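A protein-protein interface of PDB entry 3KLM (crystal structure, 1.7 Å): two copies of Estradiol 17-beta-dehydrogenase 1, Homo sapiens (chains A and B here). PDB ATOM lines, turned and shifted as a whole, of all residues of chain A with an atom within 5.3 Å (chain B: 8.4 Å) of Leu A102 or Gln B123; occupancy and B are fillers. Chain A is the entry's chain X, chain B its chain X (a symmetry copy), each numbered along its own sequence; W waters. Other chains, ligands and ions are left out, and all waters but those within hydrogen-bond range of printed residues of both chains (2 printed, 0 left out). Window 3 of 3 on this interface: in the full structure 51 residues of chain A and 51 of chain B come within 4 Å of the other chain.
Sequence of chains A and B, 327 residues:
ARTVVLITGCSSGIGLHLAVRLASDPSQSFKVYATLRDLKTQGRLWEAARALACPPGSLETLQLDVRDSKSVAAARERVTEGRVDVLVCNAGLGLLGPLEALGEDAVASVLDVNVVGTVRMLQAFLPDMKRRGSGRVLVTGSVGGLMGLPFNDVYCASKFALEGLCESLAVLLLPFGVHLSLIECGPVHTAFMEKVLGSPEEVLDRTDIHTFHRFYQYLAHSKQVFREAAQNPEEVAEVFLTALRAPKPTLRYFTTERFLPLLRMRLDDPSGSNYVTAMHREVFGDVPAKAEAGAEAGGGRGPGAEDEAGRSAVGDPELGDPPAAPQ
No position is printed for both chains.
The backbone carbonyl oxygen (O) of Leu A102 is in hydrogen-bond range of the side-chain amide nitrogen (NE2) of Gln B123, 3.0 Å away. The side-chain carboxylate of Glu A104 sits at hydrogen-bond distance from the side-chain hydroxyl of Ser B69 (2.9 Å). The side-chain carboxylate of Glu A104 lies within salt-bridge range of the guanidinium group of Arg B120. O of Leu A99 is in hydrogen-bond range of NE2 of Gln B123 (3.1 Å). The side-chain carboxylate of Glu A100 is in salt-bridge range of the side-chain amino group of Lys B130 (2.6 Å).
Printed residues of chain A that touch a printed residue of chain B: Leu A99, Glu A100, Leu A102 and Glu A104. Of the 21 printed residues of chain B, 6 touch a printed residue of chain A. Hydrophobic or aromatic side chains of chain B within 4 Å of the printed part of chain A: Val B119 and Leu B122. Among the printed residues, 7 pairs touch across the chains. Among the printed residues, Asp or Glu carboxylates within 4 Å of a Lys or Arg side-chain nitrogen of the other chain: Glu A100 with Lys B130 (2.6 Å) and Glu A104 with Arg B120 (2.9 Å).
Among the printed residues, merely in contact across the chains: Leu A99 with Leu B122 (3.7 Å) and Leu A99 with Val B119 (3.9 Å).
Of chain A, only Leu A99 (3.1 Å) and Leu A102 (3.0 Å) come within 4 Å of Gln B123. No residue of chain B comes within 4 Å of Ala A101. No residue of chain B comes within 4 Å of Gly A103. Of the printed residues of chain A, Arg B120 touches Glu A104 (2.9 Å). Of the printed residues of chain B, Leu A99 touches Val B119 (3.9 Å), Leu B122 (3.7 Å) and Gln B123 (3.1 Å). Pro B127 touches none of the printed residues of chain A. The nearest residue of chain B that does not touch Leu A102 is Val B119 (6.2 Å). The nearest residue of chain A that does not touch Gln B123 is Glu A100 (4.1 Å). The nearest printed residue of chain B that does not touch Glu A100 is Gln B123 (4.1 Å).
Water W2 lies within hydrogen-bond range of the side-chain carboxylate (OE2) of Glu A104 (2.6 Å) and the backbone NH (N) of Ser B69 (3.0 Å). Water W1 bridges the side-chain carboxylate (OE2) of Glu A100 (3.1 Å) and the side-chain amino group (NZ) of Lys B130 (3.3 Å).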
ATOM      1  N   LEU A  95     -18.858   0.955  16.092  1.00  0.00           N
ATOM      2  CA  LEU A  95     -17.854   1.450  17.003  1.00  0.00           C
ATOM      3  C   LEU A  95     -16.714   1.929  16.145  1.00  0.00           C
ATOM      4  O   LEU A  95     -16.190   1.134  15.344  1.00  0.00           O
ATOM      5  CB  LEU A  95     -17.364   0.330  17.934  1.00  0.00           C
ATOM      6  CG  LEU A  95     -16.365   0.723  19.032  1.00  0.00           C
ATOM      7  CD1 LEU A  95     -16.927   1.831  19.927  1.00  0.00           C
ATOM      8  CD2 LEU A  95     -15.970  -0.497  19.859  1.00  0.00           C
ATOM      9  N   LEU A  96     -16.369   3.222  16.263  1.00  0.00           N
ATOM     10  CA  LEU A  96     -15.475   3.848  15.314  1.00  0.00           C
ATOM     11  C   LEU A  96     -14.365   4.543  16.102  1.00  0.00           C
ATOM     12  O   LEU A  96     -14.661   5.273  17.052  1.00  0.00           O
ATOM     13  CB  LEU A  96     -16.256   4.871  14.482  1.00  0.00           C
ATOM     14  CG  LEU A  96     -15.752   5.418  13.132  1.00  0.00           C
ATOM     15  CD1 LEU A  96     -15.409   4.360  12.120  1.00  0.00           C
ATOM     16  CD2 LEU A  96     -16.837   6.362  12.534  1.00  0.00           C
ATOM     17  N   GLY A  97     -13.117   4.311  15.704  1.00  0.00           N
ATOM     18  CA  GLY A  97     -11.988   4.965  16.340  1.00  0.00           C
ATOM     19  C   GLY A  97     -10.691   4.182  16.320  1.00  0.00           C
ATOM     20  O   GLY A  97     -10.686   3.016  15.970  1.00  0.00           O
ATOM     21  N   PRO A  98      -9.569   4.822  16.712  1.00  0.00           N
ATOM     22  CA  PRO A  98      -8.298   4.147  16.853  1.00  0.00           C
ATOM     23  C   PRO A  98      -8.482   3.026  17.889  1.00  0.00           C
ATOM     24  O   PRO A  98      -9.120   3.238  18.929  1.00  0.00           O
ATOM     25  CB  PRO A  98      -7.402   5.224  17.491  1.00  0.00           C
ATOM     26  CG  PRO A  98      -8.040   6.525  17.028  1.00  0.00           C
ATOM     27  CD  PRO A  98      -9.488   6.252  17.112  1.00  0.00           C
ATOM     28  N   LEU A  99      -7.982   1.834  17.592  1.00  0.00           N
ATOM     29  CA  LEU A  99      -8.201   0.736  18.539  1.00  0.00           C
ATOM     30  C   LEU A  99      -7.836   1.094  19.974  1.00  0.00           C
ATOM     31  O   LEU A  99      -8.609   0.863  20.885  1.00  0.00           O
ATOM     32  CB  LEU A  99      -7.440  -0.509  18.113  1.00  0.00           C
ATOM     33  CG  LEU A  99      -7.657  -1.764  18.959  1.00  0.00           C
ATOM     34  CD1 LEU A  99      -8.947  -2.420  18.537  1.00  0.00           C
ATOM     35  CD2 LEU A  99      -6.467  -2.679  18.737  1.00  0.00           C
ATOM     36  N   GLU A 100      -6.672   1.699  20.180  1.00  0.00           N
ATOM     37  CA  GLU A 100      -6.227   2.022  21.558  1.00  0.00           C
ATOM     38  C   GLU A 100      -7.057   3.122  22.286  1.00  0.00           C
ATOM     39  O   GLU A 100      -6.911   3.325  23.496  1.00  0.00           O
ATOM     40  CB  GLU A 100      -4.736   2.382  21.548  1.00  0.00           C
ATOM     41  CG  GLU A 100      -4.430   3.622  20.756  1.00  0.00           C
ATOM     42  CD  GLU A 100      -4.133   3.347  19.295  1.00  0.00           C
ATOM     43  OE1 GLU A 100      -3.499   4.218  18.667  1.00  0.00           O
ATOM     44  OE2 GLU A 100      -4.527   2.293  18.751  1.00  0.00           O
ATOM     45  N   ALA A 101      -7.906   3.827  21.553  1.00  0.00           N
ATOM     46  CA  ALA A 101      -8.806   4.821  22.139  1.00  0.00           C
ATOM     47  C   ALA A 101     -10.158   4.227  22.567  1.00  0.00           C
ATOM     48  O   ALA A 101     -10.998   4.908  23.209  1.00  0.00           O
ATOM     49  CB  ALA A 101      -9.004   5.985  21.168  1.00  0.00           C
ATOM     50  N   LEU A 102     -10.411   2.961  22.214  1.00  0.00           N
ATOM     51  CA  LEU A 102     -11.714   2.372  22.513  1.00  0.00           C
ATOM     52  C   LEU A 102     -11.725   1.881  23.945  1.00  0.00           C
ATOM     53  O   LEU A 102     -10.814   1.183  24.349  1.00  0.00           O
ATOM     54  CB  LEU A 102     -11.984   1.204  21.561  1.00  0.00           C
ATOM     55  CG  LEU A 102     -11.945   1.626  20.105  1.00  0.00           C
ATOM     56  CD1 LEU A 102     -12.122   0.382  19.188  1.00  0.00           C
ATOM     57  CD2 LEU A 102     -13.004   2.651  19.860  1.00  0.00           C
ATOM     58  N   GLY A 103     -12.763   2.214  24.702  1.00  0.00           N
ATOM     59  CA  GLY A 103     -12.890   1.657  26.037  1.00  0.00           C
ATOM     60  C   GLY A 103     -13.173   0.167  25.952  1.00  0.00           C
ATOM     61  O   GLY A 103     -13.869  -0.316  25.030  1.00  0.00           O
ATOM     62  N   GLU A 104     -12.600  -0.558  26.889  1.00  0.00           N
ATOM     63  CA  GLU A 104     -12.817  -1.981  27.029  1.00  0.00           C
ATOM     64  C   GLU A 104     -14.296  -2.345  27.132  1.00  0.00           C
ATOM     65  O   GLU A 104     -14.739  -3.327  26.516  1.00  0.00           O
ATOM     66  CB  GLU A 104     -12.088  -2.454  28.288  1.00  0.00           C
ATOM     67  CG  GLU A 104     -11.762  -3.893  28.287  1.00  0.00           C
ATOM     68  CD  GLU A 104     -11.001  -4.268  29.547  1.00  0.00           C
ATOM     69  OE1 GLU A 104     -10.166  -3.442  29.997  1.00  0.00           O
ATOM     70  OE2 GLU A 104     -11.268  -5.367  30.073  1.00  0.00           O
ATOM     71  N   ALA A 106     -16.835  -0.567  25.911  1.00  0.00           N
ATOM     72  CA  ALA A 106     -17.419  -0.338  24.609  1.00  0.00           C
ATOM     73  C   ALA A 106     -17.107  -1.530  23.680  1.00  0.00           C
ATOM     74  O   ALA A 106     -17.958  -1.942  22.900  1.00  0.00           O
ATOM     75  CB  ALA A 106     -16.863   0.926  23.965  1.00  0.00           C
ATOM     76  N   VAL A 107     -15.879  -2.023  23.757  1.00  0.00           N
ATOM     77  CA  VAL A 107     -15.497  -3.208  22.939  1.00  0.00           C
ATOM     78  C   VAL A 107     -16.387  -4.398  23.334  1.00  0.00           C
ATOM     79  O   VAL A 107     -17.015  -5.022  22.495  1.00  0.00           O
ATOM     80  CB  VAL A 107     -14.031  -3.563  23.155  1.00  0.00           C
ATOM     81  CG1 VAL A 107     -13.627  -4.912  22.407  1.00  0.00           C
ATOM     82  CG2 VAL A 107     -13.152  -2.432  22.625  1.00  0.00           C
ATOM     83  N   VAL A 154     -13.082  -3.247  15.659  1.00  0.00           N
ATOM     84  CA  VAL A 154     -13.981  -4.032  16.540  1.00  0.00           C
ATOM     85  C   VAL A 154     -15.341  -4.212  15.889  1.00  0.00           C
ATOM     86  O   VAL A 154     -15.933  -5.308  15.988  1.00  0.00           O
ATOM     87  CB  VAL A 154     -14.056  -3.492  18.012  1.00  0.00           C
ATOM     88  CG1 VAL A 154     -15.203  -4.182  18.805  1.00  0.00           C
ATOM     89  CG2 VAL A 154     -12.704  -3.673  18.709  1.00  0.00           C
ATOM     90  N   SER B  69      -7.439  -6.764  31.781  1.00  0.00           N
ATOM     91  CA  SER B  69      -6.498  -5.755  31.332  1.00  0.00           C
ATOM     92  C   SER B  69      -5.451  -5.351  32.399  1.00  0.00           C
ATOM     93  O   SER B  69      -4.354  -4.915  32.042  1.00  0.00           O
ATOM     94  CB  SER B  69      -7.243  -4.552  30.803  1.00  0.00           C
ATOM     95  OG  SER B  69      -7.957  -3.949  31.860  1.00  0.00           O
ATOM     96  N   VAL B  72      -2.705  -7.935  31.896  1.00  0.00           N
ATOM     97  CA  VAL B  72      -2.003  -7.596  30.693  1.00  0.00           C
ATOM     98  C   VAL B  72      -0.984  -6.501  30.980  1.00  0.00           C
ATOM     99  O   VAL B  72       0.180  -6.613  30.606  1.00  0.00           O
ATOM    100  CB  VAL B  72      -2.996  -7.151  29.590  1.00  0.00           C
ATOM    101  CG1 VAL B  72      -2.271  -6.458  28.459  1.00  0.00           C
ATOM    102  CG2 VAL B  72      -3.841  -8.347  29.113  1.00  0.00           C
ATOM    103  N   ARG B  76       3.271  -6.668  30.904  1.00  0.00           N
ATOM    104  CA  ARG B  76       3.991  -5.698  30.070  1.00  0.00           C
ATOM    105  C   ARG B  76       5.051  -4.972  30.903  1.00  0.00           C
ATOM    106  O   ARG B  76       6.186  -4.819  30.452  1.00  0.00           O
ATOM    107  CB  ARG B  76       3.041  -4.693  29.418  1.00  0.00           C
ATOM    108  CG  ARG B  76       3.721  -3.568  28.645  1.00  0.00           C
ATOM    109  CD  ARG B  76       2.752  -2.533  28.128  1.00  0.00           C
ATOM    110  NE  ARG B  76       1.979  -1.976  29.235  1.00  0.00           N
ATOM    111  CZ  ARG B  76       0.922  -1.173  29.110  1.00  0.00           C
ATOM    112  NH1 ARG B  76       0.469  -0.812  27.911  1.00  0.00           N
ATOM    113  NH2 ARG B  76       0.309  -0.724  30.204  1.00  0.00           N
ATOM    114  N   LEU B  87       5.191  -9.702  19.126  1.00  0.00           N
ATOM    115  CA  LEU B  87       4.074 -10.059  19.997  1.00  0.00           C
ATOM    116  C   LEU B  87       3.319 -11.170  19.295  1.00  0.00           C
ATOM    117  O   LEU B  87       2.918 -11.023  18.101  1.00  0.00           O
ATOM    118  CB  LEU B  87       3.133  -8.865  20.246  1.00  0.00           C
ATOM    119  CG  LEU B  87       1.823  -9.130  20.980  1.00  0.00           C
ATOM    120  CD1 LEU B  87       2.137  -9.464  22.488  1.00  0.00           C
ATOM    121  CD2 LEU B  87       0.875  -7.911  20.849  1.00  0.00           C
ATOM    122  N   CYS B  89       0.031 -13.392  19.559  1.00  0.00           N
ATOM    123  CA  CYS B  89      -1.301 -13.469  20.158  1.00  0.00           C
ATOM    124  C   CYS B  89      -1.871 -14.830  19.787  1.00  0.00           C
ATOM    125  O   CYS B  89      -2.374 -15.037  18.662  1.00  0.00           O
ATOM    126  CB  CYS B  89      -2.190 -12.359  19.609  1.00  0.00           C
ATOM    127  SG  CYS B  89      -1.780 -10.672  20.263  1.00  0.00           S
ATOM    128  N   VAL B 116     -11.741 -10.354  22.520  1.00  0.00           N
ATOM    129  CA  VAL B 116     -11.415  -9.186  23.393  1.00  0.00           C
ATOM    130  C   VAL B 116     -10.009  -9.325  23.987  1.00  0.00           C
ATOM    131  O   VAL B 116      -9.276  -8.327  24.140  1.00  0.00           O
ATOM    132  CB  VAL B 116     -12.514  -8.939  24.492  1.00  0.00           C
ATOM    133  CG1 VAL B 116     -12.271  -7.560  25.193  1.00  0.00           C
ATOM    134  CG2 VAL B 116     -13.881  -8.942  23.876  1.00  0.00           C
ATOM    135  N   GLY B 117      -9.609 -10.534  24.362  1.00  0.00           N
ATOM    136  CA  GLY B 117      -8.252 -10.803  24.821  1.00  0.00           C
ATOM    137  C   GLY B 117      -7.161 -10.331  23.856  1.00  0.00           C
ATOM    138  O   GLY B 117      -6.193  -9.668  24.237  1.00  0.00           O
ATOM    139  N   THR B 118      -7.383 -10.576  22.574  1.00  0.00           N
ATOM    140  CA  THR B 118      -6.466 -10.083  21.570  1.00  0.00           C
ATOM    141  C   THR B 118      -6.522  -8.580  21.394  1.00  0.00           C
ATOM    142  O   THR B 118      -5.488  -7.922  21.224  1.00  0.00           O
ATOM    143  CB  THR B 118      -6.801 -10.764  20.289  1.00  0.00           C
ATOM    144  OG1 THR B 118      -6.701 -12.168  20.531  1.00  0.00           O
ATOM    145  CG2 THR B 118      -5.859 -10.306  19.184  1.00  0.00           C
ATOM    146  N   VAL B 119      -7.728  -8.017  21.408  1.00  0.00           N
ATOM    147  CA  VAL B 119      -7.871  -6.532  21.518  1.00  0.00           C
ATOM    148  C   VAL B 119      -7.060  -5.990  22.708  1.00  0.00           C
ATOM    149  O   VAL B 119      -6.282  -5.052  22.529  1.00  0.00           O
ATOM    150  CB  VAL B 119      -9.328  -6.103  21.615  1.00  0.00           C
ATOM    151  CG1 VAL B 119      -9.394  -4.582  21.738  1.00  0.00           C
ATOM    152  CG2 VAL B 119     -10.051  -6.475  20.348  1.00  0.00           C
ATOM    153  N   ARG B 120      -7.214  -6.548  23.916  1.00  0.00           N
ATOM    154  CA  ARG B 120      -6.433  -6.043  25.092  1.00  0.00           C
ATOM    155  C   ARG B 120      -4.936  -6.058  24.885  1.00  0.00           C
ATOM    156  O   ARG B 120      -4.224  -5.098  25.265  1.00  0.00           O
ATOM    157  CB  ARG B 120      -6.767  -6.802  26.370  1.00  0.00           C
ATOM    158  CG  ARG B 120      -8.249  -6.648  26.787  1.00  0.00           C
ATOM    159  CD  ARG B 120      -8.452  -7.398  28.109  1.00  0.00           C
ATOM    160  NE  ARG B 120      -9.852  -7.295  28.511  1.00  0.00           N
ATOM    161  CZ  ARG B 120     -10.766  -8.245  28.303  1.00  0.00           C
ATOM    162  NH1 ARG B 120     -10.431  -9.374  27.673  1.00  0.00           N
ATOM    163  NH2 ARG B 120     -12.024  -8.069  28.709  1.00  0.00           N
ATOM    164  N   MET B 121      -4.408  -7.136  24.288  1.00  0.00           N
ATOM    165  CA  MET B 121      -2.983  -7.217  23.970  1.00  0.00           C
ATOM    166  C   MET B 121      -2.528  -6.169  22.950  1.00  0.00           C
ATOM    167  O   MET B 121      -1.485  -5.543  23.128  1.00  0.00           O
ATOM    168  CB  MET B 121      -2.625  -8.607  23.443  1.00  0.00           C
ATOM    169  CG  MET B 121      -2.836  -9.793  24.389  1.00  0.00           C
ATOM    170  SD  MET B 121      -1.898  -9.627  25.946  1.00  0.00           S
ATOM    171  CE  MET B 121      -0.227  -9.789  25.328  1.00  0.00           C
ATOM    172  N   LEU B 122      -3.270  -6.018  21.863  1.00  0.00           N
ATOM    173  CA  LEU B 122      -2.981  -4.993  20.866  1.00  0.00           C
ATOM    174  C   LEU B 122      -3.098  -3.569  21.461  1.00  0.00           C
ATOM    175  O   LEU B 122      -2.225  -2.726  21.193  1.00  0.00           O
ATOM    176  CB  LEU B 122      -3.908  -5.166  19.660  1.00  0.00           C
ATOM    177  CG  LEU B 122      -3.647  -6.491  18.916  1.00  0.00           C
ATOM    178  CD1 LEU B 122      -4.797  -6.802  17.952  1.00  0.00           C
ATOM    179  CD2 LEU B 122      -2.294  -6.497  18.219  1.00  0.00           C
ATOM    180  N   GLN B 123      -4.084  -3.305  22.331  1.00  0.00           N
ATOM    181  CA  GLN B 123      -4.172  -1.949  22.926  1.00  0.00           C
ATOM    182  C   GLN B 123      -2.955  -1.676  23.794  1.00  0.00           C
ATOM    183  O   GLN B 123      -2.448  -0.523  23.817  1.00  0.00           O
ATOM    184  CB  GLN B 123      -5.438  -1.786  23.793  1.00  0.00           C
ATOM    185  CG  GLN B 123      -6.699  -1.837  22.983  1.00  0.00           C
ATOM    186  CD  GLN B 123      -7.929  -1.729  23.815  1.00  0.00           C
ATOM    187  OE1 GLN B 123      -8.077  -2.411  24.838  1.00  0.00           O
ATOM    188  NE2 GLN B 123      -8.841  -0.883  23.380  1.00  0.00           N
ATOM    189  N   ALA B 124      -2.543  -2.692  24.570  1.00  0.00           N
ATOM    190  CA  ALA B 124      -1.408  -2.594  25.461  1.00  0.00           C
ATOM    191  C   ALA B 124      -0.094  -2.426  24.706  1.00  0.00           C
ATOM    192  O   ALA B 124       0.745  -1.611  25.121  1.00  0.00           O
ATOM    193  CB  ALA B 124      -1.330  -3.767  26.440  1.00  0.00           C
ATOM    194  N   PHE B 125       0.098  -3.174  23.609  1.00  0.00           N
ATOM    195  CA  PHE B 125       1.426  -3.259  22.969  1.00  0.00           C
ATOM    196  C   PHE B 125       1.622  -2.480  21.692  1.00  0.00           C
ATOM    197  O   PHE B 125       2.763  -2.113  21.407  1.00  0.00           O
ATOM    198  CB  PHE B 125       1.866  -4.728  22.775  1.00  0.00           C
ATOM    199  CG  PHE B 125       2.169  -5.453  24.081  1.00  0.00           C
ATOM    200  CD1 PHE B 125       3.461  -5.443  24.615  1.00  0.00           C
ATOM    201  CD2 PHE B 125       1.172  -6.102  24.799  1.00  0.00           C
ATOM    202  CE1 PHE B 125       3.762  -6.091  25.785  1.00  0.00           C
ATOM    203  CE2 PHE B 125       1.456  -6.750  26.005  1.00  0.00           C
ATOM    204  CZ  PHE B 125       2.747  -6.748  26.511  1.00  0.00           C
ATOM    205  N   LEU B 126       0.569  -2.232  20.910  1.00  0.00           N
ATOM    206  CA  LEU B 126       0.720  -1.478  19.644  1.00  0.00           C
ATOM    207  C   LEU B 126       1.256  -0.042  19.793  1.00  0.00           C
ATOM    208  O   LEU B 126       2.054   0.407  18.946  1.00  0.00           O
ATOM    209  CB  LEU B 126      -0.574  -1.418  18.813  1.00  0.00           C
ATOM    210  CG  LEU B 126      -1.009  -2.654  18.069  1.00  0.00           C
ATOM    211  CD1 LEU B 126      -2.440  -2.404  17.473  1.00  0.00           C
ATOM    212  CD2 LEU B 126       0.042  -3.073  16.991  1.00  0.00           C
ATOM    213  N   PRO B 127       0.785   0.707  20.806  1.00  0.00           N
ATOM    214  CA  PRO B 127       1.295   2.090  20.918  1.00  0.00           C
ATOM    215  C   PRO B 127       2.838   2.242  20.877  1.00  0.00           C
ATOM    216  O   PRO B 127       3.349   3.060  20.063  1.00  0.00           O
ATOM    217  CB  PRO B 127       0.708   2.563  22.251  1.00  0.00           C
ATOM    218  CG  PRO B 127      -0.594   1.802  22.349  1.00  0.00           C
ATOM    219  CD  PRO B 127      -0.217   0.418  21.849  1.00  0.00           C
ATOM    220  N   ASP B 128       3.576   1.491  21.700  1.00  0.00           N
ATOM    221  CA  ASP B 128       5.043   1.628  21.687  1.00  0.00           C
ATOM    222  C   ASP B 128       5.644   1.150  20.357  1.00  0.00           C
ATOM    223  O   ASP B 128       6.678   1.647  19.938  1.00  0.00           O
ATOM    224  CB  ASP B 128       5.744   0.950  22.877  1.00  0.00           C
ATOM    225  CG  ASP B 128       7.297   1.185  22.864  1.00  0.00           C
ATOM    226  OD1 ASP B 128       8.084   0.210  22.891  1.00  0.00           O
ATOM    227  OD2 ASP B 128       7.739   2.363  22.780  1.00  0.00           O
ATOM    228  N   LYS B 130       4.140   1.542  17.371  1.00  0.00           N
ATOM    229  CA  LYS B 130       3.841   2.602  16.386  1.00  0.00           C
ATOM    230  C   LYS B 130       4.816   3.752  16.599  1.00  0.00           C
ATOM    231  O   LYS B 130       5.248   4.376  15.632  1.00  0.00           O
ATOM    232  CB  LYS B 130       2.410   3.127  16.541  1.00  0.00           C
ATOM    233  CG  LYS B 130       1.324   2.155  16.101  1.00  0.00           C
ATOM    234  CD  LYS B 130       0.010   2.519  16.772  1.00  0.00           C
ATOM    235  CE  LYS B 130      -0.906   3.253  15.825  1.00  0.00           C
ATOM    236  NZ  LYS B 130      -2.120   3.760  16.544  1.00  0.00           N
ATOM    237  N   LEU B 165     -10.658  -8.222  12.689  1.00  0.00           N
ATOM    238  CA  LEU B 165      -9.862  -7.344  13.549  1.00  0.00           C
ATOM    239  C   LEU B 165      -8.498  -7.056  12.915  1.00  0.00           C
ATOM    240  O   LEU B 165      -8.103  -5.902  12.758  1.00  0.00           O
ATOM    241  CB  LEU B 165      -9.606  -7.999  14.929  1.00  0.00           C
ATOM    242  CG  LEU B 165      -8.744  -7.235  15.950  1.00  0.00           C
ATOM    243  CD1 LEU B 165      -9.476  -5.965  16.350  1.00  0.00           C
ATOM    244  CD2 LEU B 165      -8.481  -8.084  17.159  1.00  0.00           C
ATOM    245  N   LEU B 169      -6.922  -3.574  11.101  1.00  0.00           N
ATOM    246  CA  LEU B 169      -5.676  -3.014  11.659  1.00  0.00           C
ATOM    247  C   LEU B 169      -4.540  -2.944  10.650  1.00  0.00           C
ATOM    248  O   LEU B 169      -3.825  -1.901  10.601  1.00  0.00           O
ATOM    249  CB  LEU B 169      -5.203  -3.770  12.922  1.00  0.00           C
ATOM    250  CG  LEU B 169      -5.922  -3.546  14.244  1.00  0.00           C
ATOM    251  CD1 LEU B 169      -5.526  -4.654  15.162  1.00  0.00           C
ATOM    252  CD2 LEU B 169      -5.543  -2.200  14.800  1.00  0.00           C
HETATM  253  O   HOH W   1      -5.015   2.414  15.728  1.00  0.00           O
HETATM  254  O   HOH W   2     -10.396  -6.361  32.365  1.00  0.00           O
